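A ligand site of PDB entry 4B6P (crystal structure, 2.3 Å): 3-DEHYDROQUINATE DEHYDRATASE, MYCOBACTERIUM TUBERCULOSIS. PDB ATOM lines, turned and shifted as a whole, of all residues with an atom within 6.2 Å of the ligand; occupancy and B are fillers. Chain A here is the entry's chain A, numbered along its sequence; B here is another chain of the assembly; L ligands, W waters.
An oxygen (O5) of the ligand sits at hydrogen-bond distance from the side-chain carboxylate (OD2) of Asp 88 of chain B, 2.5 Å away.
The backbone NH (N) of Ser 103 lies within hydrogen-bond range of an oxygen (O3) of the ligand.
The side-chain hydroxyl of Ser 103 lies within hydrogen-bond range of an oxygen (O3) of the ligand.
NE2 of His 81 is in hydrogen-bond range of O6 of the ligand (2.7 Å).
The side-chain amide oxygen (OD1) of Asn 75 is in hydrogen-bond range of an oxygen (O1) of the ligand, 2.7 Å away.
The backbone NH (N) of Ile 102 lies within hydrogen-bond range of an oxygen (O2) of the ligand, at 2.8 Å.
A ring nitrogen (ND1) of His 101 is in hydrogen-bond range of an oxygen (O1) of the ligand (2.9 Å).
O5 of the ligand is in hydrogen-bond range of NH1 of Arg 112 (3.0 Å).
The backbone NH of Gly 78 lies within hydrogen-bond range of an oxygen (O5) of the ligand (3.3 Å).
The guanidinium group of Arg 19 lies within hydrogen-bond range of the backbone carbonyl oxygen of Asp 88 of chain B.
The side-chain carboxylate of Asp 88 of chain B lies within salt-bridge range of the guanidinium group of Arg 112 (3.0 Å).
The backbone NH of Gly 77 sits close to the side-chain amide oxygen of Asn 75 (3.3 Å).
OD1 of Asn 75 lies close to O of Val 100, at 3.4 Å.
ND2 of Asn 12 is in hydrogen-bond range of O of Ala 85 of chain B (2.8 Å).
NH1 of Arg 19 lies within salt-bridge range of OE1 of Glu 92 of chain B, at 3.2 Å.
OE1 of Glu 20 lies within salt-bridge range of NE of Arg 19 (3.3 Å).
The backbone carbonyl oxygen of Gly 77 lies within hydrogen-bond range of the side-chain hydroxyl of Thr 80.
A fluorine (F3) of the ligand sits close to the backbone carbonyl oxygen of Asn 12 (2.7 Å).
NH1 of Arg 19 sits close to F4 of the ligand, at 2.9 Å.
A fluorine (F5) of the ligand lies close to the side-chain hydroxyl (OH) of Tyr 24 (3.3 Å).
Residues that only touch the ligand: Pro 11 (3.8 Å), Leu 13 (3.4 Å), Arg 15 (3.6 Å), Leu 16 (3.5 Å), Gly 77 (3.1 Å), Val 105 (3.8 Å) and Val 84 of chain B (3.9 Å).
Of the 32 residues printed, 18 come within 4 Å of the ligand.
Water W2 lies within hydrogen-bond range of the side-chain carboxylate of Asp 88 of chain B (2.7 Å), the guanidinium group of Arg 108 (3.2 Å) and the guanidinium group of Arg 112 (3.5 Å).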
ATOM      1  N   PRO A  11     -30.321 -17.775  25.264  1.00  0.00           N
ATOM      2  CA  PRO A  11     -30.313 -17.362  23.872  1.00  0.00           C
ATOM      3  C   PRO A  11     -29.943 -18.424  22.865  1.00  0.00           C
ATOM      4  O   PRO A  11     -28.978 -19.181  23.062  1.00  0.00           O
ATOM      5  CB  PRO A  11     -29.241 -16.291  23.841  1.00  0.00           C
ATOM      6  CG  PRO A  11     -29.226 -15.728  25.144  1.00  0.00           C
ATOM      7  CD  PRO A  11     -29.577 -16.827  26.107  1.00  0.00           C
ATOM      8  N   ASN A  12     -30.726 -18.457  21.783  1.00  0.00           N
ATOM      9  CA  ASN A  12     -30.487 -19.328  20.636  1.00  0.00           C
ATOM     10  C   ASN A  12     -30.882 -20.787  20.803  1.00  0.00           C
ATOM     11  O   ASN A  12     -30.812 -21.550  19.834  1.00  0.00           O
ATOM     12  CB  ASN A  12     -29.038 -19.196  20.172  1.00  0.00           C
ATOM     13  CG  ASN A  12     -28.729 -17.807  19.646  1.00  0.00           C
ATOM     14  OD1 ASN A  12     -29.396 -17.338  18.728  1.00  0.00           O
ATOM     15  ND2 ASN A  12     -27.735 -17.162  20.196  1.00  0.00           N
ATOM     16  N   LEU A  13     -31.295 -21.197  22.013  1.00  0.00           N
ATOM     17  CA  LEU A  13     -31.719 -22.579  22.228  1.00  0.00           C
ATOM     18  C   LEU A  13     -33.074 -22.884  21.598  1.00  0.00           C
ATOM     19  O   LEU A  13     -33.373 -24.038  21.332  1.00  0.00           O
ATOM     20  CB  LEU A  13     -31.729 -22.962  23.707  1.00  0.00           C
ATOM     21  CG  LEU A  13     -30.380 -23.533  24.262  1.00  0.00           C
ATOM     22  CD1 LEU A  13     -30.027 -24.898  23.655  1.00  0.00           C
ATOM     23  CD2 LEU A  13     -29.231 -22.554  24.124  1.00  0.00           C
ATOM     24  N   GLY A  14     -33.875 -21.850  21.310  1.00  0.00           N
ATOM     25  CA  GLY A  14     -35.078 -22.026  20.473  1.00  0.00           C
ATOM     26  C   GLY A  14     -34.787 -22.379  19.007  1.00  0.00           C
ATOM     27  O   GLY A  14     -35.652 -22.840  18.275  1.00  0.00           O
ATOM     28  N   ARG A  15     -33.539 -22.199  18.580  1.00  0.00           N
ATOM     29  CA  ARG A  15     -33.108 -22.531  17.225  1.00  0.00           C
ATOM     30  C   ARG A  15     -32.590 -23.956  17.087  1.00  0.00           C
ATOM     31  O   ARG A  15     -32.226 -24.408  15.991  1.00  0.00           O
ATOM     32  CB  ARG A  15     -32.020 -21.578  16.793  1.00  0.00           C
ATOM     33  CG  ARG A  15     -32.416 -20.151  16.887  1.00  0.00           C
ATOM     34  CD  ARG A  15     -33.541 -19.828  15.953  1.00  0.00           C
ATOM     35  NE  ARG A  15     -33.104 -19.971  14.575  1.00  0.00           N
ATOM     36  CZ  ARG A  15     -33.865 -19.840  13.511  1.00  0.00           C
ATOM     37  NH1 ARG A  15     -35.173 -19.542  13.642  1.00  0.00           N
ATOM     38  NH2 ARG A  15     -33.311 -20.003  12.302  1.00  0.00           N
ATOM     39  N   LEU A  16     -32.558 -24.662  18.200  1.00  0.00           N
ATOM     40  CA  LEU A  16     -32.183 -26.051  18.220  1.00  0.00           C
ATOM     41  C   LEU A  16     -32.985 -26.835  17.159  1.00  0.00           C
ATOM     42  O   LEU A  16     -34.185 -26.579  16.965  1.00  0.00           O
ATOM     43  CB  LEU A  16     -32.496 -26.559  19.614  1.00  0.00           C
ATOM     44  CG  LEU A  16     -31.961 -27.860  20.130  1.00  0.00           C
ATOM     45  CD1 LEU A  16     -30.401 -27.922  20.037  1.00  0.00           C
ATOM     46  CD2 LEU A  16     -32.518 -27.916  21.557  1.00  0.00           C
ATOM     47  N   GLY A  17     -32.322 -27.757  16.456  1.00  0.00           N
ATOM     48  CA  GLY A  17     -32.997 -28.575  15.431  1.00  0.00           C
ATOM     49  C   GLY A  17     -33.225 -27.836  14.113  1.00  0.00           C
ATOM     50  O   GLY A  17     -33.982 -28.270  13.244  1.00  0.00           O
ATOM     51  N   ARG A  19     -30.585 -24.967  11.660  1.00  0.00           N
ATOM     52  CA  ARG A  19     -29.264 -24.387  11.749  1.00  0.00           C
ATOM     53  C   ARG A  19     -28.097 -25.359  11.459  1.00  0.00           C
ATOM     54  O   ARG A  19     -27.453 -25.221  10.395  1.00  0.00           O
ATOM     55  CB  ARG A  19     -29.087 -23.636  13.109  1.00  0.00           C
ATOM     56  CG  ARG A  19     -28.845 -24.404  14.419  1.00  0.00           C
ATOM     57  CD  ARG A  19     -28.461 -23.442  15.537  1.00  0.00           C
ATOM     58  NE  ARG A  19     -27.172 -22.764  15.330  1.00  0.00           N
ATOM     59  CZ  ARG A  19     -26.940 -21.450  15.480  1.00  0.00           C
ATOM     60  NH1 ARG A  19     -27.915 -20.596  15.855  1.00  0.00           N
ATOM     61  NH2 ARG A  19     -25.708 -20.971  15.259  1.00  0.00           N
ATOM     62  N   GLU A  20     -27.869 -26.346  12.343  1.00  0.00           N
ATOM     63  CA  GLU A  20     -26.620 -27.141  12.360  1.00  0.00           C
ATOM     64  C   GLU A  20     -26.853 -28.635  12.774  1.00  0.00           C
ATOM     65  O   GLU A  20     -26.370 -29.070  13.849  1.00  0.00           O
ATOM     66  CB  GLU A  20     -25.551 -26.433  13.248  1.00  0.00           C
ATOM     67  CG  GLU A  20     -24.811 -25.213  12.526  1.00  0.00           C
ATOM     68  CD  GLU A  20     -24.259 -24.094  13.441  1.00  0.00           C
ATOM     69  OE1 GLU A  20     -24.262 -24.226  14.688  1.00  0.00           O
ATOM     70  OE2 GLU A  20     -23.811 -23.073  12.867  1.00  0.00           O
ATOM     71  N   TYR A  24     -25.600 -30.146  16.983  1.00  0.00           N
ATOM     72  CA  TYR A  24     -26.403 -30.229  18.222  1.00  0.00           C
ATOM     73  C   TYR A  24     -27.524 -31.301  18.208  1.00  0.00           C
ATOM     74  O   TYR A  24     -28.172 -31.541  19.219  1.00  0.00           O
ATOM     75  CB  TYR A  24     -27.043 -28.870  18.527  1.00  0.00           C
ATOM     76  CG  TYR A  24     -26.111 -27.676  18.492  1.00  0.00           C
ATOM     77  CD1 TYR A  24     -25.107 -27.528  19.432  1.00  0.00           C
ATOM     78  CD2 TYR A  24     -26.260 -26.678  17.530  1.00  0.00           C
ATOM     79  CE1 TYR A  24     -24.257 -26.450  19.410  1.00  0.00           C
ATOM     80  CE2 TYR A  24     -25.409 -25.560  17.500  1.00  0.00           C
ATOM     81  CZ  TYR A  24     -24.414 -25.460  18.449  1.00  0.00           C
ATOM     82  OH  TYR A  24     -23.555 -24.383  18.470  1.00  0.00           O
ATOM     83  N   ASN A  75     -29.037 -24.065  30.784  1.00  0.00           N
ATOM     84  CA  ASN A  75     -28.216 -23.906  29.602  1.00  0.00           C
ATOM     85  C   ASN A  75     -28.346 -22.468  29.166  1.00  0.00           C
ATOM     86  O   ASN A  75     -29.276 -22.110  28.417  1.00  0.00           O
ATOM     87  CB  ASN A  75     -28.641 -24.853  28.501  1.00  0.00           C
ATOM     88  CG  ASN A  75     -27.712 -24.826  27.338  1.00  0.00           C
ATOM     89  OD1 ASN A  75     -26.893 -23.903  27.208  1.00  0.00           O
ATOM     90  ND2 ASN A  75     -27.814 -25.843  26.462  1.00  0.00           N
ATOM     91  N   ALA A  76     -27.451 -21.609  29.653  1.00  0.00           N
ATOM     92  CA  ALA A  76     -27.594 -20.161  29.388  1.00  0.00           C
ATOM     93  C   ALA A  76     -27.207 -19.728  27.969  1.00  0.00           C
ATOM     94  O   ALA A  76     -27.260 -18.541  27.668  1.00  0.00           O
ATOM     95  CB  ALA A  76     -26.812 -19.332  30.431  1.00  0.00           C
ATOM     96  N   GLY A  77     -26.824 -20.630  27.081  1.00  0.00           N
ATOM     97  CA  GLY A  77     -26.373 -20.233  25.746  1.00  0.00           C
ATOM     98  C   GLY A  77     -25.122 -19.360  25.836  1.00  0.00           C
ATOM     99  O   GLY A  77     -24.291 -19.558  26.722  1.00  0.00           O
ATOM    100  N   GLY A  78     -25.054 -18.331  24.995  1.00  0.00           N
ATOM    101  CA  GLY A  78     -23.906 -17.435  24.946  1.00  0.00           C
ATOM    102  C   GLY A  78     -23.618 -16.693  26.226  1.00  0.00           C
ATOM    103  O   GLY A  78     -22.463 -16.321  26.471  1.00  0.00           O
ATOM    104  N   LEU A  79     -24.673 -16.457  27.019  1.00  0.00           N
ATOM    105  CA  LEU A  79     -24.569 -15.707  28.274  1.00  0.00           C
ATOM    106  C   LEU A  79     -23.728 -16.481  29.320  1.00  0.00           C
ATOM    107  O   LEU A  79     -23.256 -15.918  30.322  1.00  0.00           O
ATOM    108  CB  LEU A  79     -25.970 -15.452  28.820  1.00  0.00           C
ATOM    109  CG  LEU A  79     -26.912 -14.558  28.004  1.00  0.00           C
ATOM    110  CD1 LEU A  79     -28.257 -14.429  28.724  1.00  0.00           C
ATOM    111  CD2 LEU A  79     -26.298 -13.195  27.781  1.00  0.00           C
ATOM    112  N   THR A  80     -23.590 -17.788  29.094  1.00  0.00           N
ATOM    113  CA  THR A  80     -22.703 -18.631  29.890  1.00  0.00           C
ATOM    114  C   THR A  80     -21.363 -17.965  30.027  1.00  0.00           C
ATOM    115  O   THR A  80     -20.805 -17.951  31.108  1.00  0.00           O
ATOM    116  CB  THR A  80     -22.505 -19.982  29.206  1.00  0.00           C
ATOM    117  OG1 THR A  80     -23.778 -20.609  29.021  1.00  0.00           O
ATOM    118  CG2 THR A  80     -21.571 -20.880  30.037  1.00  0.00           C
ATOM    119  N   HIS A  81     -20.864 -17.380  28.937  1.00  0.00           N
ATOM    120  CA  HIS A  81     -19.484 -16.943  28.834  1.00  0.00           C
ATOM    121  C   HIS A  81     -19.328 -15.462  29.134  1.00  0.00           C
ATOM    122  O   HIS A  81     -18.203 -14.968  29.252  1.00  0.00           O
ATOM    123  CB  HIS A  81     -18.944 -17.250  27.415  1.00  0.00           C
ATOM    124  CG  HIS A  81     -19.298 -18.620  26.945  1.00  0.00           C
ATOM    125  ND1 HIS A  81     -18.867 -19.760  27.575  1.00  0.00           N
ATOM    126  CD2 HIS A  81     -20.117 -19.026  25.951  1.00  0.00           C
ATOM    127  CE1 HIS A  81     -19.364 -20.816  26.961  1.00  0.00           C
ATOM    128  NE2 HIS A  81     -20.125 -20.393  25.968  1.00  0.00           N
ATOM    129  N   VAL A 100     -25.644 -27.151  31.978  1.00  0.00           N
ATOM    130  CA  VAL A 100     -25.696 -28.138  30.890  1.00  0.00           C
ATOM    131  C   VAL A 100     -25.414 -27.430  29.583  1.00  0.00           C
ATOM    132  O   VAL A 100     -25.969 -26.380  29.319  1.00  0.00           O
ATOM    133  CB  VAL A 100     -27.042 -28.862  30.793  1.00  0.00           C
ATOM    134  CG1 VAL A 100     -27.126 -29.626  29.484  1.00  0.00           C
ATOM    135  CG2 VAL A 100     -27.260 -29.827  32.018  1.00  0.00           C
ATOM    136  N   HIS A 101     -24.519 -28.000  28.807  1.00  0.00           N
ATOM    137  CA  HIS A 101     -24.278 -27.590  27.414  1.00  0.00           C
ATOM    138  C   HIS A 101     -24.383 -28.820  26.502  1.00  0.00           C
ATOM    139  O   HIS A 101     -23.815 -29.893  26.786  1.00  0.00           O
ATOM    140  CB  HIS A 101     -22.919 -26.869  27.281  1.00  0.00           C
ATOM    141  CG  HIS A 101     -22.818 -25.679  28.179  1.00  0.00           C
ATOM    142  ND1 HIS A 101     -23.544 -24.527  27.958  1.00  0.00           N
ATOM    143  CD2 HIS A 101     -22.127 -25.477  29.323  1.00  0.00           C
ATOM    144  CE1 HIS A 101     -23.320 -23.670  28.930  1.00  0.00           C
ATOM    145  NE2 HIS A 101     -22.439 -24.207  29.757  1.00  0.00           N
ATOM    146  N   ILE A 102     -25.131 -28.647  25.424  1.00  0.00           N
ATOM    147  CA  ILE A 102     -25.349 -29.705  24.464  1.00  0.00           C
ATOM    148  C   ILE A 102     -23.998 -30.058  23.783  1.00  0.00           C
ATOM    149  O   ILE A 102     -23.578 -31.227  23.782  1.00  0.00           O
ATOM    150  CB  ILE A 102     -26.457 -29.311  23.452  1.00  0.00           C
ATOM    151  CG1 ILE A 102     -27.810 -29.119  24.165  1.00  0.00           C
ATOM    152  CG2 ILE A 102     -26.572 -30.378  22.354  1.00  0.00           C
ATOM    153  CD1 ILE A 102     -28.876 -28.567  23.268  1.00  0.00           C
ATOM    154  N   SER A 103     -23.313 -29.038  23.243  1.00  0.00           N
ATOM    155  CA  SER A 103     -22.014 -29.235  22.607  1.00  0.00           C
ATOM    156  C   SER A 103     -20.873 -29.334  23.648  1.00  0.00           C
ATOM    157  O   SER A 103     -21.014 -28.919  24.820  1.00  0.00           O
ATOM    158  CB  SER A 103     -21.732 -28.085  21.630  1.00  0.00           C
ATOM    159  OG  SER A 103     -21.451 -26.840  22.287  1.00  0.00           O
ATOM    160  N   ASN A 104     -19.739 -29.913  23.232  1.00  0.00           N
ATOM    161  CA  ASN A 104     -18.540 -29.887  24.070  1.00  0.00           C
ATOM    162  C   ASN A 104     -17.846 -28.533  23.933  1.00  0.00           C
ATOM    163  O   ASN A 104     -17.068 -28.323  23.006  1.00  0.00           O
ATOM    164  CB  ASN A 104     -17.572 -31.026  23.716  1.00  0.00           C
ATOM    165  CG  ASN A 104     -16.428 -31.136  24.702  1.00  0.00           C
ATOM    166  OD1 ASN A 104     -16.164 -30.195  25.464  1.00  0.00           O
ATOM    167  ND2 ASN A 104     -15.728 -32.268  24.701  1.00  0.00           N
ATOM    168  N   VAL A 105     -18.144 -27.624  24.860  1.00  0.00           N
ATOM    169  CA  VAL A 105     -17.613 -26.253  24.811  1.00  0.00           C
ATOM    170  C   VAL A 105     -16.065 -26.212  24.841  1.00  0.00           C
ATOM    171  O   VAL A 105     -15.452 -25.252  24.367  1.00  0.00           O
ATOM    172  CB  VAL A 105     -18.210 -25.339  25.975  1.00  0.00           C
ATOM    173  CG1 VAL A 105     -19.763 -25.216  25.868  1.00  0.00           C
ATOM    174  CG2 VAL A 105     -17.842 -25.860  27.313  1.00  0.00           C
ATOM    175  N   ARG A 108     -14.203 -26.221  21.198  1.00  0.00           N
ATOM    176  CA  ARG A 108     -14.575 -25.135  20.315  1.00  0.00           C
ATOM    177  C   ARG A 108     -13.598 -23.975  20.535  1.00  0.00           C
ATOM    178  O   ARG A 108     -12.412 -24.232  20.823  1.00  0.00           O
ATOM    179  CB  ARG A 108     -16.033 -24.762  20.625  1.00  0.00           C
ATOM    180  CG  ARG A 108     -17.007 -25.933  20.350  1.00  0.00           C
ATOM    181  CD  ARG A 108     -18.451 -25.545  20.657  1.00  0.00           C
ATOM    182  NE  ARG A 108     -18.953 -24.636  19.630  1.00  0.00           N
ATOM    183  CZ  ARG A 108     -20.213 -24.285  19.486  1.00  0.00           C
ATOM    184  NH1 ARG A 108     -21.154 -24.718  20.304  1.00  0.00           N
ATOM    185  NH2 ARG A 108     -20.545 -23.480  18.488  1.00  0.00           N
ATOM    186  N   PHE A 111     -12.791 -18.878  23.935  1.00  0.00           N
ATOM    187  CA  PHE A 111     -13.726 -18.084  24.729  1.00  0.00           C
ATOM    188  C   PHE A 111     -14.859 -18.879  25.352  1.00  0.00           C
ATOM    189  O   PHE A 111     -15.380 -18.453  26.379  1.00  0.00           O
ATOM    190  CB  PHE A 111     -14.275 -16.862  23.969  1.00  0.00           C
ATOM    191  CG  PHE A 111     -15.123 -17.172  22.773  1.00  0.00           C
ATOM    192  CD1 PHE A 111     -16.462 -17.504  22.908  1.00  0.00           C
ATOM    193  CD2 PHE A 111     -14.614 -16.991  21.499  1.00  0.00           C
ATOM    194  CE1 PHE A 111     -17.234 -17.735  21.787  1.00  0.00           C
ATOM    195  CE2 PHE A 111     -15.390 -17.203  20.389  1.00  0.00           C
ATOM    196  CZ  PHE A 111     -16.688 -17.576  20.519  1.00  0.00           C
ATOM    197  N   ARG A 112     -15.234 -20.011  24.745  1.00  0.00           N
ATOM    198  CA  ARG A 112     -16.253 -20.917  25.280  1.00  0.00           C
ATOM    199  C   ARG A 112     -15.810 -21.834  26.436  1.00  0.00           C
ATOM    200  O   ARG A 112     -16.621 -22.491  27.076  1.00  0.00           O
ATOM    201  CB  ARG A 112     -16.815 -21.777  24.147  1.00  0.00           C
ATOM    202  CG  ARG A 112     -17.508 -20.970  23.065  1.00  0.00           C
ATOM    203  CD  ARG A 112     -18.273 -21.888  22.099  1.00  0.00           C
ATOM    204  NE  ARG A 112     -18.499 -21.185  20.839  1.00  0.00           N
ATOM    205  CZ  ARG A 112     -19.536 -20.396  20.574  1.00  0.00           C
ATOM    206  NH1 ARG A 112     -20.526 -20.220  21.476  1.00  0.00           N
ATOM    207  NH2 ARG A 112     -19.594 -19.786  19.399  1.00  0.00           N
ATOM    208  N   TYR A 133     -29.420 -33.118  29.690  1.00  0.00           N
ATOM    209  CA  TYR A 133     -30.572 -32.636  30.457  1.00  0.00           C
ATOM    210  C   TYR A 133     -31.223 -33.764  31.251  1.00  0.00           C
ATOM    211  O   TYR A 133     -31.596 -33.592  32.396  1.00  0.00           O
ATOM    212  CB  TYR A 133     -31.629 -32.066  29.549  1.00  0.00           C
ATOM    213  CG  TYR A 133     -31.266 -30.750  28.888  1.00  0.00           C
ATOM    214  CD1 TYR A 133     -31.494 -29.543  29.542  1.00  0.00           C
ATOM    215  CD2 TYR A 133     -30.749 -30.718  27.609  1.00  0.00           C
ATOM    216  CE1 TYR A 133     -31.198 -28.335  28.937  1.00  0.00           C
ATOM    217  CE2 TYR A 133     -30.452 -29.513  26.990  1.00  0.00           C
ATOM    218  CZ  TYR A 133     -30.684 -28.328  27.661  1.00  0.00           C
ATOM    219  OH  TYR A 133     -30.393 -27.136  27.016  1.00  0.00           O
ATOM    220  N   VAL B  84     -21.551 -13.092  22.872  1.00  0.00           N
ATOM    221  CA  VAL B  84     -21.412 -14.418  22.246  1.00  0.00           C
ATOM    222  C   VAL B  84     -22.776 -14.874  21.682  1.00  0.00           C
ATOM    223  O   VAL B  84     -22.849 -15.431  20.599  1.00  0.00           O
ATOM    224  CB  VAL B  84     -20.780 -15.463  23.228  1.00  0.00           C
ATOM    225  CG1 VAL B  84     -20.813 -16.910  22.639  1.00  0.00           C
ATOM    226  CG2 VAL B  84     -19.353 -15.038  23.621  1.00  0.00           C
ATOM    227  N   ALA B  85     -23.856 -14.569  22.394  1.00  0.00           N
ATOM    228  CA  ALA B  85     -25.232 -14.885  21.931  1.00  0.00           C
ATOM    229  C   ALA B  85     -25.498 -14.365  20.497  1.00  0.00           C
ATOM    230  O   ALA B  85     -26.030 -15.076  19.616  1.00  0.00           O
ATOM    231  CB  ALA B  85     -26.282 -14.342  22.922  1.00  0.00           C
ATOM    232  N   ASP B  88     -23.504 -16.376  17.939  1.00  0.00           N
ATOM    233  CA  ASP B  88     -24.136 -17.661  17.726  1.00  0.00           C
ATOM    234  C   ASP B  88     -25.332 -17.525  16.768  1.00  0.00           C
ATOM    235  O   ASP B  88     -25.526 -18.351  15.914  1.00  0.00           O
ATOM    236  CB  ASP B  88     -24.656 -18.218  19.047  1.00  0.00           C
ATOM    237  CG  ASP B  88     -23.561 -18.667  19.983  1.00  0.00           C
ATOM    238  OD1 ASP B  88     -22.468 -19.032  19.508  1.00  0.00           O
ATOM    239  OD2 ASP B  88     -23.843 -18.667  21.225  1.00  0.00           O
ATOM    240  N   ALA B  89     -26.148 -16.492  16.942  1.00  0.00           N
ATOM    241  CA  ALA B  89     -27.303 -16.272  16.057  1.00  0.00           C
ATOM    242  C   ALA B  89     -26.854 -16.026  14.636  1.00  0.00           C
ATOM    243  O   ALA B  89     -27.434 -16.574  13.691  1.00  0.00           O
ATOM    244  CB  ALA B  89     -28.118 -15.093  16.548  1.00  0.00           C
ATOM    245  N   GLU B  92     -25.524 -18.788  12.030  1.00  0.00           N
ATOM    246  CA  GLU B  92     -26.574 -19.471  11.239  1.00  0.00           C
ATOM    247  C   GLU B  92     -26.814 -18.898   9.860  1.00  0.00           C
ATOM    248  O   GLU B  92     -27.362 -19.550   8.989  1.00  0.00           O
ATOM    249  CB  GLU B  92     -27.933 -19.333  11.934  1.00  0.00           C
ATOM    250  CG  GLU B  92     -28.484 -20.585  12.362  1.00  0.00           C
ATOM    251  CD  GLU B  92     -29.916 -20.461  12.775  1.00  0.00           C
ATOM    252  OE1 GLU B  92     -30.150 -19.707  13.737  1.00  0.00           O
ATOM    253  OE2 GLU B  92     -30.771 -21.129  12.136  1.00  0.00           O
HETATM  254  F1  LIG L   1     -27.521 -25.383  21.479  1.00  0.00           F
HETATM  255  C1  LIG L   1     -27.261 -24.303  20.731  1.00  0.00           C
HETATM  256  C2  LIG L   1     -28.220 -23.911  19.828  1.00  0.00           C
HETATM  257  F2  LIG L   1     -29.356 -24.606  19.707  1.00  0.00           F
HETATM  258  C3  LIG L   1     -27.959 -22.793  19.059  1.00  0.00           C
HETATM  259  F3  LIG L   1     -28.782 -22.310  18.152  1.00  0.00           F
HETATM  260  C4  LIG L   1     -26.798 -22.096  19.166  1.00  0.00           C
HETATM  261  F4  LIG L   1     -26.660 -21.029  18.385  1.00  0.00           F
HETATM  262  C5  LIG L   1     -25.831 -22.484  20.054  1.00  0.00           C
HETATM  263  F5  LIG L   1     -24.698 -21.729  20.090  1.00  0.00           F
HETATM  264  C6  LIG L   1     -26.060 -23.601  20.854  1.00  0.00           C
HETATM  265  C7  LIG L   1     -25.003 -24.046  21.838  1.00  0.00           C
HETATM  266  C8  LIG L   1     -25.138 -23.384  23.206  1.00  0.00           C
HETATM  267  C9  LIG L   1     -24.255 -24.072  24.252  1.00  0.00           C
HETATM  268  O1  LIG L   1     -24.769 -23.591  25.507  1.00  0.00           O
HETATM  269  C10 LIG L   1     -24.508 -25.583  24.155  1.00  0.00           C
HETATM  270  O2  LIG L   1     -25.575 -25.945  24.635  1.00  0.00           O
HETATM  271  O3  LIG L   1     -23.683 -26.316  23.523  1.00  0.00           O
HETATM  272  C11 LIG L   1     -24.757 -21.918  23.087  1.00  0.00           C
HETATM  273  O4  LIG L   1     -25.656 -21.098  22.903  1.00  0.00           O
HETATM  274  C12 LIG L   1     -23.256 -21.531  23.066  1.00  0.00           C
HETATM  275  O5  LIG L   1     -23.026 -20.117  23.123  1.00  0.00           O
HETATM  276  C13 LIG L   1     -22.486 -22.266  24.194  1.00  0.00           C
HETATM  277  O6  LIG L   1     -21.093 -21.996  24.003  1.00  0.00           O
HETATM  278  C14 LIG L   1     -22.736 -23.769  24.075  1.00  0.00           C
HETATM  279  O   HOH W   1     -26.385 -18.406  22.520  1.00  0.00           O
HETATM  280  O   HOH W   2     -22.369 -20.969  17.659  1.00  0.00           O
